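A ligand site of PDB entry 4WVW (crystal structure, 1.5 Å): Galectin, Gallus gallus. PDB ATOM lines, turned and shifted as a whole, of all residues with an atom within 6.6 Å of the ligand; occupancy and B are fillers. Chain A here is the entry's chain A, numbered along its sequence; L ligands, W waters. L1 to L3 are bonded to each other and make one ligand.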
ATOM      1  N   ARG A  36      33.255  16.805  25.051  1.00  0.00           N
ATOM      2  CA  ARG A  36      32.358  17.224  23.988  1.00  0.00           C
ATOM      3  C   ARG A  36      32.887  18.508  23.363  1.00  0.00           C
ATOM      4  O   ARG A  36      33.726  19.198  23.956  1.00  0.00           O
ATOM      5  CB  ARG A  36      30.955  17.483  24.543  1.00  0.00           C
ATOM      6  CG  ARG A  36      30.907  18.488  25.679  1.00  0.00           C
ATOM      7  CD  ARG A  36      29.471  18.877  26.012  1.00  0.00           C
ATOM      8  NE  ARG A  36      28.951  19.889  25.088  1.00  0.00           N
ATOM      9  CZ  ARG A  36      27.663  20.126  24.905  1.00  0.00           C
ATOM     10  NH1 ARG A  36      26.757  19.412  25.557  1.00  0.00           N
ATOM     11  NH2 ARG A  36      27.266  21.072  24.064  1.00  0.00           N
ATOM     12  N   GLN A  38      31.319  21.690  20.242  1.00  0.00           N
ATOM     13  CA  GLN A  38      30.210  22.034  19.368  1.00  0.00           C
ATOM     14  C   GLN A  38      30.614  23.049  18.310  1.00  0.00           C
ATOM     15  O   GLN A  38      31.474  23.896  18.544  1.00  0.00           O
ATOM     16  CB  GLN A  38      29.000  22.549  20.145  1.00  0.00           C
ATOM     17  CG  GLN A  38      29.171  23.949  20.728  1.00  0.00           C
ATOM     18  CD  GLN A  38      28.396  24.125  22.010  1.00  0.00           C
ATOM     19  OE1 GLN A  38      28.656  23.430  23.005  1.00  0.00           O
ATOM     20  NE2 GLN A  38      27.433  25.051  22.016  1.00  0.00           N
ATOM     21  N   ASP A  40      28.536  25.769  16.077  1.00  0.00           N
ATOM     22  CA  ASP A  40      27.237  26.463  16.067  1.00  0.00           C
ATOM     23  C   ASP A  40      27.166  27.479  14.929  1.00  0.00           C
ATOM     24  O   ASP A  40      28.026  28.342  14.811  1.00  0.00           O
ATOM     25  CB  ASP A  40      26.982  27.175  17.403  1.00  0.00           C
ATOM     26  CG  ASP A  40      26.805  26.221  18.583  1.00  0.00           C
ATOM     27  OD1 ASP A  40      26.503  25.028  18.359  1.00  0.00           O
ATOM     28  OD2 ASP A  40      26.943  26.679  19.747  1.00  0.00           O
ATOM     29  N   ARG A  50      20.864  35.098  24.690  1.00  0.00           N
ATOM     30  CA  ARG A  50      21.749  34.286  23.895  1.00  0.00           C
ATOM     31  C   ARG A  50      21.338  34.217  22.436  1.00  0.00           C
ATOM     32  O   ARG A  50      20.159  34.010  22.114  1.00  0.00           O
ATOM     33  CB  ARG A  50      21.836  32.881  24.470  1.00  0.00           C
ATOM     34  CG  ARG A  50      22.839  32.015  23.764  1.00  0.00           C
ATOM     35  CD  ARG A  50      22.867  30.645  24.364  1.00  0.00           C
ATOM     36  NE  ARG A  50      23.667  29.735  23.554  1.00  0.00           N
ATOM     37  CZ  ARG A  50      23.819  28.452  23.837  1.00  0.00           C
ATOM     38  NH1 ARG A  50      23.232  27.937  24.902  1.00  0.00           N
ATOM     39  NH2 ARG A  50      24.579  27.688  23.050  1.00  0.00           N
ATOM     40  N   VAL A  53      20.776  29.766  17.651  1.00  0.00           N
ATOM     41  CA  VAL A  53      21.663  28.841  16.960  1.00  0.00           C
ATOM     42  C   VAL A  53      20.838  28.065  15.942  1.00  0.00           C
ATOM     43  O   VAL A  53      20.026  27.215  16.295  1.00  0.00           O
ATOM     44  CB  VAL A  53      22.321  27.860  17.936  1.00  0.00           C
ATOM     45  CG1 VAL A  53      23.224  26.892  17.163  1.00  0.00           C
ATOM     46  CG2 VAL A  53      23.115  28.628  18.988  1.00  0.00           C
ATOM     47  N   HIS A  56      23.230  23.547  15.653  1.00  0.00           N
ATOM     48  CA  HIS A  56      24.130  23.137  16.734  1.00  0.00           C
ATOM     49  C   HIS A  56      24.565  21.731  16.383  1.00  0.00           C
ATOM     50  O   HIS A  56      23.717  20.828  16.302  1.00  0.00           O
ATOM     51  CB  HIS A  56      23.313  23.133  18.025  1.00  0.00           C
ATOM     52  CG  HIS A  56      24.020  22.607  19.245  1.00  0.00           C
ATOM     53  ND1 HIS A  56      25.086  23.271  19.837  1.00  0.00           N
ATOM     54  CD2 HIS A  56      23.742  21.564  20.045  1.00  0.00           C
ATOM     55  CE1 HIS A  56      25.435  22.632  20.936  1.00  0.00           C
ATOM     56  NE2 HIS A  56      24.643  21.584  21.094  1.00  0.00           N
ATOM     57  N   ASN A  58      26.997  18.838  17.746  1.00  0.00           N
ATOM     58  CA  ASN A  58      27.570  18.615  19.080  1.00  0.00           C
ATOM     59  C   ASN A  58      27.980  17.161  19.330  1.00  0.00           C
ATOM     60  O   ASN A  58      27.223  16.367  19.896  1.00  0.00           O
ATOM     61  CB  ASN A  58      26.571  19.121  20.135  1.00  0.00           C
ATOM     62  CG  ASN A  58      26.969  18.790  21.578  1.00  0.00           C
ATOM     63  OD1 ASN A  58      26.095  18.535  22.406  1.00  0.00           O
ATOM     64  ND2 ASN A  58      28.265  18.817  21.884  1.00  0.00           N
ATOM     65  N   ARG A  60      29.550  14.219  21.331  1.00  0.00           N
ATOM     66  CA  ARG A  60      29.696  13.912  22.757  1.00  0.00           C
ATOM     67  C   ARG A  60      30.394  12.574  22.876  1.00  0.00           C
ATOM     68  O   ARG A  60      29.943  11.582  22.296  1.00  0.00           O
ATOM     69  CB  ARG A  60      28.322  13.833  23.428  1.00  0.00           C
ATOM     70  CG  ARG A  60      27.570  15.154  23.386  1.00  0.00           C
ATOM     71  CD  ARG A  60      26.182  15.029  23.969  1.00  0.00           C
ATOM     72  NE  ARG A  60      25.479  16.312  23.881  1.00  0.00           N
ATOM     73  CZ  ARG A  60      24.297  16.568  24.435  1.00  0.00           C
ATOM     74  NH1 ARG A  60      23.659  15.632  25.136  1.00  0.00           N
ATOM     75  NH2 ARG A  60      23.761  17.771  24.293  1.00  0.00           N
ATOM     76  N   VAL A  68      24.842  15.077  18.768  1.00  0.00           N
ATOM     77  CA  VAL A  68      23.544  15.724  18.976  1.00  0.00           C
ATOM     78  C   VAL A  68      23.439  16.943  18.091  1.00  0.00           C
ATOM     79  O   VAL A  68      24.334  17.786  18.070  1.00  0.00           O
ATOM     80  CB  VAL A  68      23.367  16.132  20.458  1.00  0.00           C
ATOM     81  CG1 VAL A  68      22.064  16.905  20.647  1.00  0.00           C
ATOM     82  CG2 VAL A  68      23.402  14.891  21.366  1.00  0.00           C
ATOM     83  N   CYS A  69      22.342  17.051  17.328  1.00  0.00           N
ATOM     84  CA  CYS A  69      22.087  18.278  16.589  1.00  0.00           C
ATOM     85  C   CYS A  69      20.782  18.903  17.061  1.00  0.00           C
ATOM     86  O   CYS A  69      19.852  18.191  17.442  1.00  0.00           O
ATOM     87  CB  CYS A  69      22.024  18.024  15.077  1.00  0.00           C
ATOM     88  SG  CYS A  69      23.544  17.399  14.364  1.00  0.00           S
ATOM     89  N   ASN A  70      20.736  20.231  17.057  1.00  0.00           N
ATOM     90  CA  ASN A  70      19.558  20.922  17.542  1.00  0.00           C
ATOM     91  C   ASN A  70      19.587  22.365  17.065  1.00  0.00           C
ATOM     92  O   ASN A  70      20.524  22.783  16.380  1.00  0.00           O
ATOM     93  CB  ASN A  70      19.511  20.870  19.084  1.00  0.00           C
ATOM     94  CG  ASN A  70      18.100  20.954  19.641  1.00  0.00           C
ATOM     95  OD1 ASN A  70      17.150  21.288  18.939  1.00  0.00           O
ATOM     96  ND2 ASN A  70      17.961  20.638  20.926  1.00  0.00           N
ATOM     97  N   THR A  71      18.551  23.096  17.437  1.00  0.00           N
ATOM     98  CA  THR A  71      18.410  24.504  17.086  1.00  0.00           C
ATOM     99  C   THR A  71      17.995  25.218  18.356  1.00  0.00           C
ATOM    100  O   THR A  71      17.133  24.717  19.094  1.00  0.00           O
ATOM    101  CB  THR A  71      17.309  24.686  16.022  1.00  0.00           C
ATOM    102  OG1 THR A  71      17.799  24.164  14.764  1.00  0.00           O
ATOM    103  CG2 THR A  71      16.965  26.144  15.839  1.00  0.00           C
ATOM    104  N   LEU A  72      18.619  26.371  18.640  1.00  0.00           N
ATOM    105  CA  LEU A  72      18.234  27.193  19.780  1.00  0.00           C
ATOM    106  C   LEU A  72      17.544  28.428  19.247  1.00  0.00           C
ATOM    107  O   LEU A  72      18.110  29.152  18.418  1.00  0.00           O
ATOM    108  CB  LEU A  72      19.463  27.596  20.596  1.00  0.00           C
ATOM    109  CG  LEU A  72      19.185  28.445  21.830  1.00  0.00           C
ATOM    110  CD1 LEU A  72      18.935  27.553  23.025  1.00  0.00           C
ATOM    111  CD2 LEU A  72      20.368  29.340  22.109  1.00  0.00           C
ATOM    112  N   TRP A  77      16.173  25.436  23.559  1.00  0.00           N
ATOM    113  CA  TRP A  77      16.555  24.340  22.689  1.00  0.00           C
ATOM    114  C   TRP A  77      15.312  23.618  22.179  1.00  0.00           C
ATOM    115  O   TRP A  77      14.331  23.462  22.927  1.00  0.00           O
ATOM    116  CB  TRP A  77      17.459  23.349  23.435  1.00  0.00           C
ATOM    117  CG  TRP A  77      18.878  23.841  23.601  1.00  0.00           C
ATOM    118  CD1 TRP A  77      19.504  24.191  24.763  1.00  0.00           C
ATOM    119  CD2 TRP A  77      19.826  24.055  22.554  1.00  0.00           C
ATOM    120  NE1 TRP A  77      20.782  24.613  24.510  1.00  0.00           N
ATOM    121  CE2 TRP A  77      21.008  24.547  23.160  1.00  0.00           C
ATOM    122  CE3 TRP A  77      19.799  23.882  21.165  1.00  0.00           C
ATOM    123  CZ2 TRP A  77      22.153  24.837  22.417  1.00  0.00           C
ATOM    124  CZ3 TRP A  77      20.918  24.195  20.437  1.00  0.00           C
ATOM    125  CH2 TRP A  77      22.086  24.675  21.052  1.00  0.00           C
ATOM    126  N   GLY A  78      15.356  23.177  20.931  1.00  0.00           N
ATOM    127  CA  GLY A  78      14.286  22.407  20.349  1.00  0.00           C
ATOM    128  C   GLY A  78      14.458  20.917  20.589  1.00  0.00           C
ATOM    129  O   GLY A  78      15.163  20.500  21.512  1.00  0.00           O
ATOM    130  N   TRP A  79      13.823  20.110  19.760  1.00  0.00           N
ATOM    131  CA  TRP A  79      13.937  18.669  19.881  1.00  0.00           C
ATOM    132  C   TRP A  79      15.225  18.195  19.241  1.00  0.00           C
ATOM    133  O   TRP A  79      15.512  18.507  18.093  1.00  0.00           O
ATOM    134  CB  TRP A  79      12.736  17.971  19.261  1.00  0.00           C
ATOM    135  CG  TRP A  79      11.469  18.223  20.025  1.00  0.00           C
ATOM    136  CD1 TRP A  79      11.364  18.829  21.243  1.00  0.00           C
ATOM    137  CD2 TRP A  79      10.144  17.885  19.614  1.00  0.00           C
ATOM    138  NE1 TRP A  79      10.040  18.885  21.618  1.00  0.00           N
ATOM    139  CE2 TRP A  79       9.266  18.316  20.641  1.00  0.00           C
ATOM    140  CE3 TRP A  79       9.604  17.261  18.490  1.00  0.00           C
ATOM    141  CZ2 TRP A  79       7.889  18.142  20.563  1.00  0.00           C
ATOM    142  CZ3 TRP A  79       8.228  17.092  18.421  1.00  0.00           C
ATOM    143  CH2 TRP A  79       7.387  17.520  19.455  1.00  0.00           C
ATOM    144  N   GLU A  80      16.006  17.443  20.007  1.00  0.00           N
ATOM    145  CA  GLU A  80      17.285  16.921  19.519  1.00  0.00           C
ATOM    146  C   GLU A  80      17.130  15.878  18.426  1.00  0.00           C
ATOM    147  O   GLU A  80      16.208  15.049  18.444  1.00  0.00           O
ATOM    148  CB  GLU A  80      18.079  16.316  20.675  1.00  0.00           C
ATOM    149  CG  GLU A  80      18.543  17.363  21.680  1.00  0.00           C
ATOM    150  CD  GLU A  80      19.251  16.769  22.878  1.00  0.00           C
ATOM    151  OE1 GLU A  80      19.170  15.536  23.117  1.00  0.00           O
ATOM    152  OE2 GLU A  80      19.892  17.561  23.600  1.00  0.00           O
ATOM    153  N   ILE A  82      19.571  12.971  17.295  1.00  0.00           N
ATOM    154  CA  ILE A  82      20.791  12.314  17.744  1.00  0.00           C
ATOM    155  C   ILE A  82      21.223  11.247  16.759  1.00  0.00           C
ATOM    156  O   ILE A  82      20.436  10.372  16.391  1.00  0.00           O
ATOM    157  CB  ILE A  82      20.598  11.706  19.146  1.00  0.00           C
ATOM    158  CG1 ILE A  82      20.102  12.765  20.134  1.00  0.00           C
ATOM    159  CG2 ILE A  82      21.897  11.060  19.644  1.00  0.00           C
ATOM    160  CD1 ILE A  82      19.893  12.250  21.547  1.00  0.00           C
ATOM    161  N   TYR A 132      33.111  25.793  20.174  1.00  0.00           N
ATOM    162  CA  TYR A 132      33.317  25.814  21.613  1.00  0.00           C
ATOM    163  C   TYR A 132      33.612  24.420  22.136  1.00  0.00           C
ATOM    164  O   TYR A 132      33.253  23.418  21.501  1.00  0.00           O
ATOM    165  CB  TYR A 132      32.055  26.324  22.322  1.00  0.00           C
ATOM    166  CG  TYR A 132      31.387  27.552  21.743  1.00  0.00           C
ATOM    167  CD1 TYR A 132      31.724  28.826  22.183  1.00  0.00           C
ATOM    168  CD2 TYR A 132      30.393  27.432  20.785  1.00  0.00           C
ATOM    169  CE1 TYR A 132      31.102  29.943  21.666  1.00  0.00           C
ATOM    170  CE2 TYR A 132      29.751  28.545  20.274  1.00  0.00           C
ATOM    171  CZ  TYR A 132      30.109  29.799  20.720  1.00  0.00           C
ATOM    172  OH  TYR A 132      29.488  30.917  20.203  1.00  0.00           O
HETATM  173  C1  LIG L   1      18.447  16.973  28.306  1.00  0.00           C
HETATM  174  C2  LIG L   1      19.216  16.564  27.068  1.00  0.00           C
HETATM  175  C3  LIG L   1      20.568  17.165  26.972  1.00  0.00           C
HETATM  176  C4  LIG L   1      20.542  18.624  27.158  1.00  0.00           C
HETATM  177  C5  LIG L   1      19.979  18.909  28.484  1.00  0.00           C
HETATM  178  C6  LIG L   1      19.795  20.353  28.772  1.00  0.00           C
HETATM  179  O1  LIG L   1      18.890  16.253  29.398  1.00  0.00           O
HETATM  180  O2  LIG L   1      19.330  15.174  27.071  1.00  0.00           O
HETATM  181  O3  LIG L   1      21.113  16.805  25.699  1.00  0.00           O
HETATM  182  O4  LIG L   1      21.878  19.154  27.079  1.00  0.00           O
HETATM  183  O5  LIG L   1      18.587  18.344  28.590  1.00  0.00           O
HETATM  184  O6  LIG L   1      19.027  21.071  27.816  1.00  0.00           O
HETATM  185  C1  LG2 L   2      21.997  20.283  26.238  1.00  0.00           C
HETATM  186  C2  LG2 L   2      23.357  20.865  26.458  1.00  0.00           C
HETATM  187  C3  LG2 L   2      23.671  21.992  25.529  1.00  0.00           C
HETATM  188  C4  LG2 L   2      23.361  21.659  24.169  1.00  0.00           C
HETATM  189  C5  LG2 L   2      21.971  21.103  24.031  1.00  0.00           C
HETATM  190  C6  LG2 L   2      21.578  20.664  22.671  1.00  0.00           C
HETATM  191  O1  LG2 L   2      23.460  21.310  27.783  1.00  0.00           O
HETATM  192  O2  LG2 L   2      25.095  22.266  25.798  1.00  0.00           O
HETATM  193  O3  LG2 L   2      24.326  20.690  23.682  1.00  0.00           O
HETATM  194  O4  LG2 L   2      21.791  19.921  24.910  1.00  0.00           O
HETATM  195  O5  LG2 L   2      20.350  20.086  22.575  1.00  0.00           O
HETATM  196  C1  LG3 L   3      24.749  24.874  25.218  1.00  0.00           C
HETATM  197  C2  LG3 L   3      25.539  23.690  25.935  1.00  0.00           C
HETATM  198  C3  LG3 L   3      27.030  23.867  26.107  1.00  0.00           C
HETATM  199  C4  LG3 L   3      27.381  24.935  26.960  1.00  0.00           C
HETATM  200  C5  LG3 L   3      26.701  24.945  28.210  1.00  0.00           C
HETATM  201  C6  LG3 L   3      25.216  24.853  28.004  1.00  0.00           C
HETATM  202  C7  LG3 L   3      24.458  24.843  29.358  1.00  0.00           C
HETATM  203  C8  LG3 L   3      22.992  24.491  29.171  1.00  0.00           C
HETATM  204  C9  LG3 L   3      22.175  24.669  30.459  1.00  0.00           C
HETATM  205  C10 LG3 L   3      27.769  26.243  30.159  1.00  0.00           C
HETATM  206  C11 LG3 L   3      28.112  27.582  30.815  1.00  0.00           C
HETATM  207  N1  LG3 L   3      27.054  26.232  28.903  1.00  0.00           N
HETATM  208  O1  LG3 L   3      23.582  25.222  25.549  1.00  0.00           O
HETATM  209  O2  LG3 L   3      25.320  25.371  24.199  1.00  0.00           O
HETATM  210  O3  LG3 L   3      28.846  24.916  27.216  1.00  0.00           O
HETATM  211  O4  LG3 L   3      24.750  23.832  27.123  1.00  0.00           O
HETATM  212  O5  LG3 L   3      25.012  23.941  30.230  1.00  0.00           O
HETATM  213  O6  LG3 L   3      22.480  25.320  28.217  1.00  0.00           O
HETATM  214  O7  LG3 L   3      22.274  25.904  31.096  1.00  0.00           O
HETATM  215  O8  LG3 L   3      28.092  25.193  30.713  1.00  0.00           O
HETATM  216  O   HOH W   1      22.915  28.477  28.576  1.00  0.00           O
HETATM  217  O   HOH W   2      29.798  22.266  28.094  1.00  0.00           O
HETATM  218  O   HOH W   3      20.406  13.868  24.813  1.00  0.00           O
HETATM  219  O   HOH W   4      29.771  25.426  24.807  1.00  0.00           O
HETATM  220  O   HOH W   5      19.391  23.759  28.228  1.00  0.00           O
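Of the 19 residues printed, 9 come within 4 Å of the ligand.
Along chain A the residues within 4 Å of the ligand span positions 36 to 80.
Water W4 lies within hydrogen-bond range of an oxygen (O3) of LG3 L3 (2.6 Å) and the side-chain amide oxygen (OE1) of Gln 38 (2.9 Å).
Water W3 bridges the side-chain carboxylate (OE1) of Glu 80 (2.7 Å) and an oxygen (O2) of LIG L1 (2.8 Å).
O2 of LG3 L3 sits at hydrogen-bond distance from NE2 of Gln 38, 3.1 Å away.
The indole nitrogen (NE1) of Trp 77 is in hydrogen-bond range of an oxygen (O1) of LG3 L3 (3.0 Å).
An oxygen (O3) of LG2 L2 sits at hydrogen-bond distance from the guanidinium group (NH2) of Arg 36 (3.0 Å).
ND2 of Asn 70 sits at hydrogen-bond distance from O5 of LG2 L2 (3.0 Å).
An oxygen (O3) of LIG L1 sits at hydrogen-bond distance from the side-chain carboxylate of Glu 80, 2.5 Å away.
An oxygen (O3) of LG2 L2 lies within hydrogen-bond range of the side-chain amide oxygen (OD1) of Asn 58, at 3.1 Å.
NE2 of His 56 is in hydrogen-bond range of O3 of LG2 L2 (2.8 Å).
O2 of LG3 L3 is in salt-bridge range of NH2 of Arg 50, 2.7 Å away.
An oxygen (O3) of LIG L1 lies within hydrogen-bond range of the guanidinium group (NH1) of Arg 60, at 2.9 Å.
A ring nitrogen (ND1) of His 56 lies within hydrogen-bond range of the side-chain carboxylate (OD1) of Asp 40.
OD1 of Asn 70 lies close to O of Trp 79 (3.3 Å).
N of His 56 lies within hydrogen-bond range of O of Asn 70 (2.9 Å).
ND2 of Asn 70 is in hydrogen-bond range of O of Gly 78 (2.9 Å).
OE1 of Gln 38 sits at hydrogen-bond distance from NH2 of Arg 36.
The guanidinium group of Arg 60 is in salt-bridge range of the side-chain carboxylate of Glu 80.
The side-chain amide nitrogen of Gln 38 sits at hydrogen-bond distance from the side-chain carboxylate of Asp 40 (2.8 Å).
NH2 of Arg 36 sits at hydrogen-bond distance from OD1 of Asn 58, at 3.2 Å.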
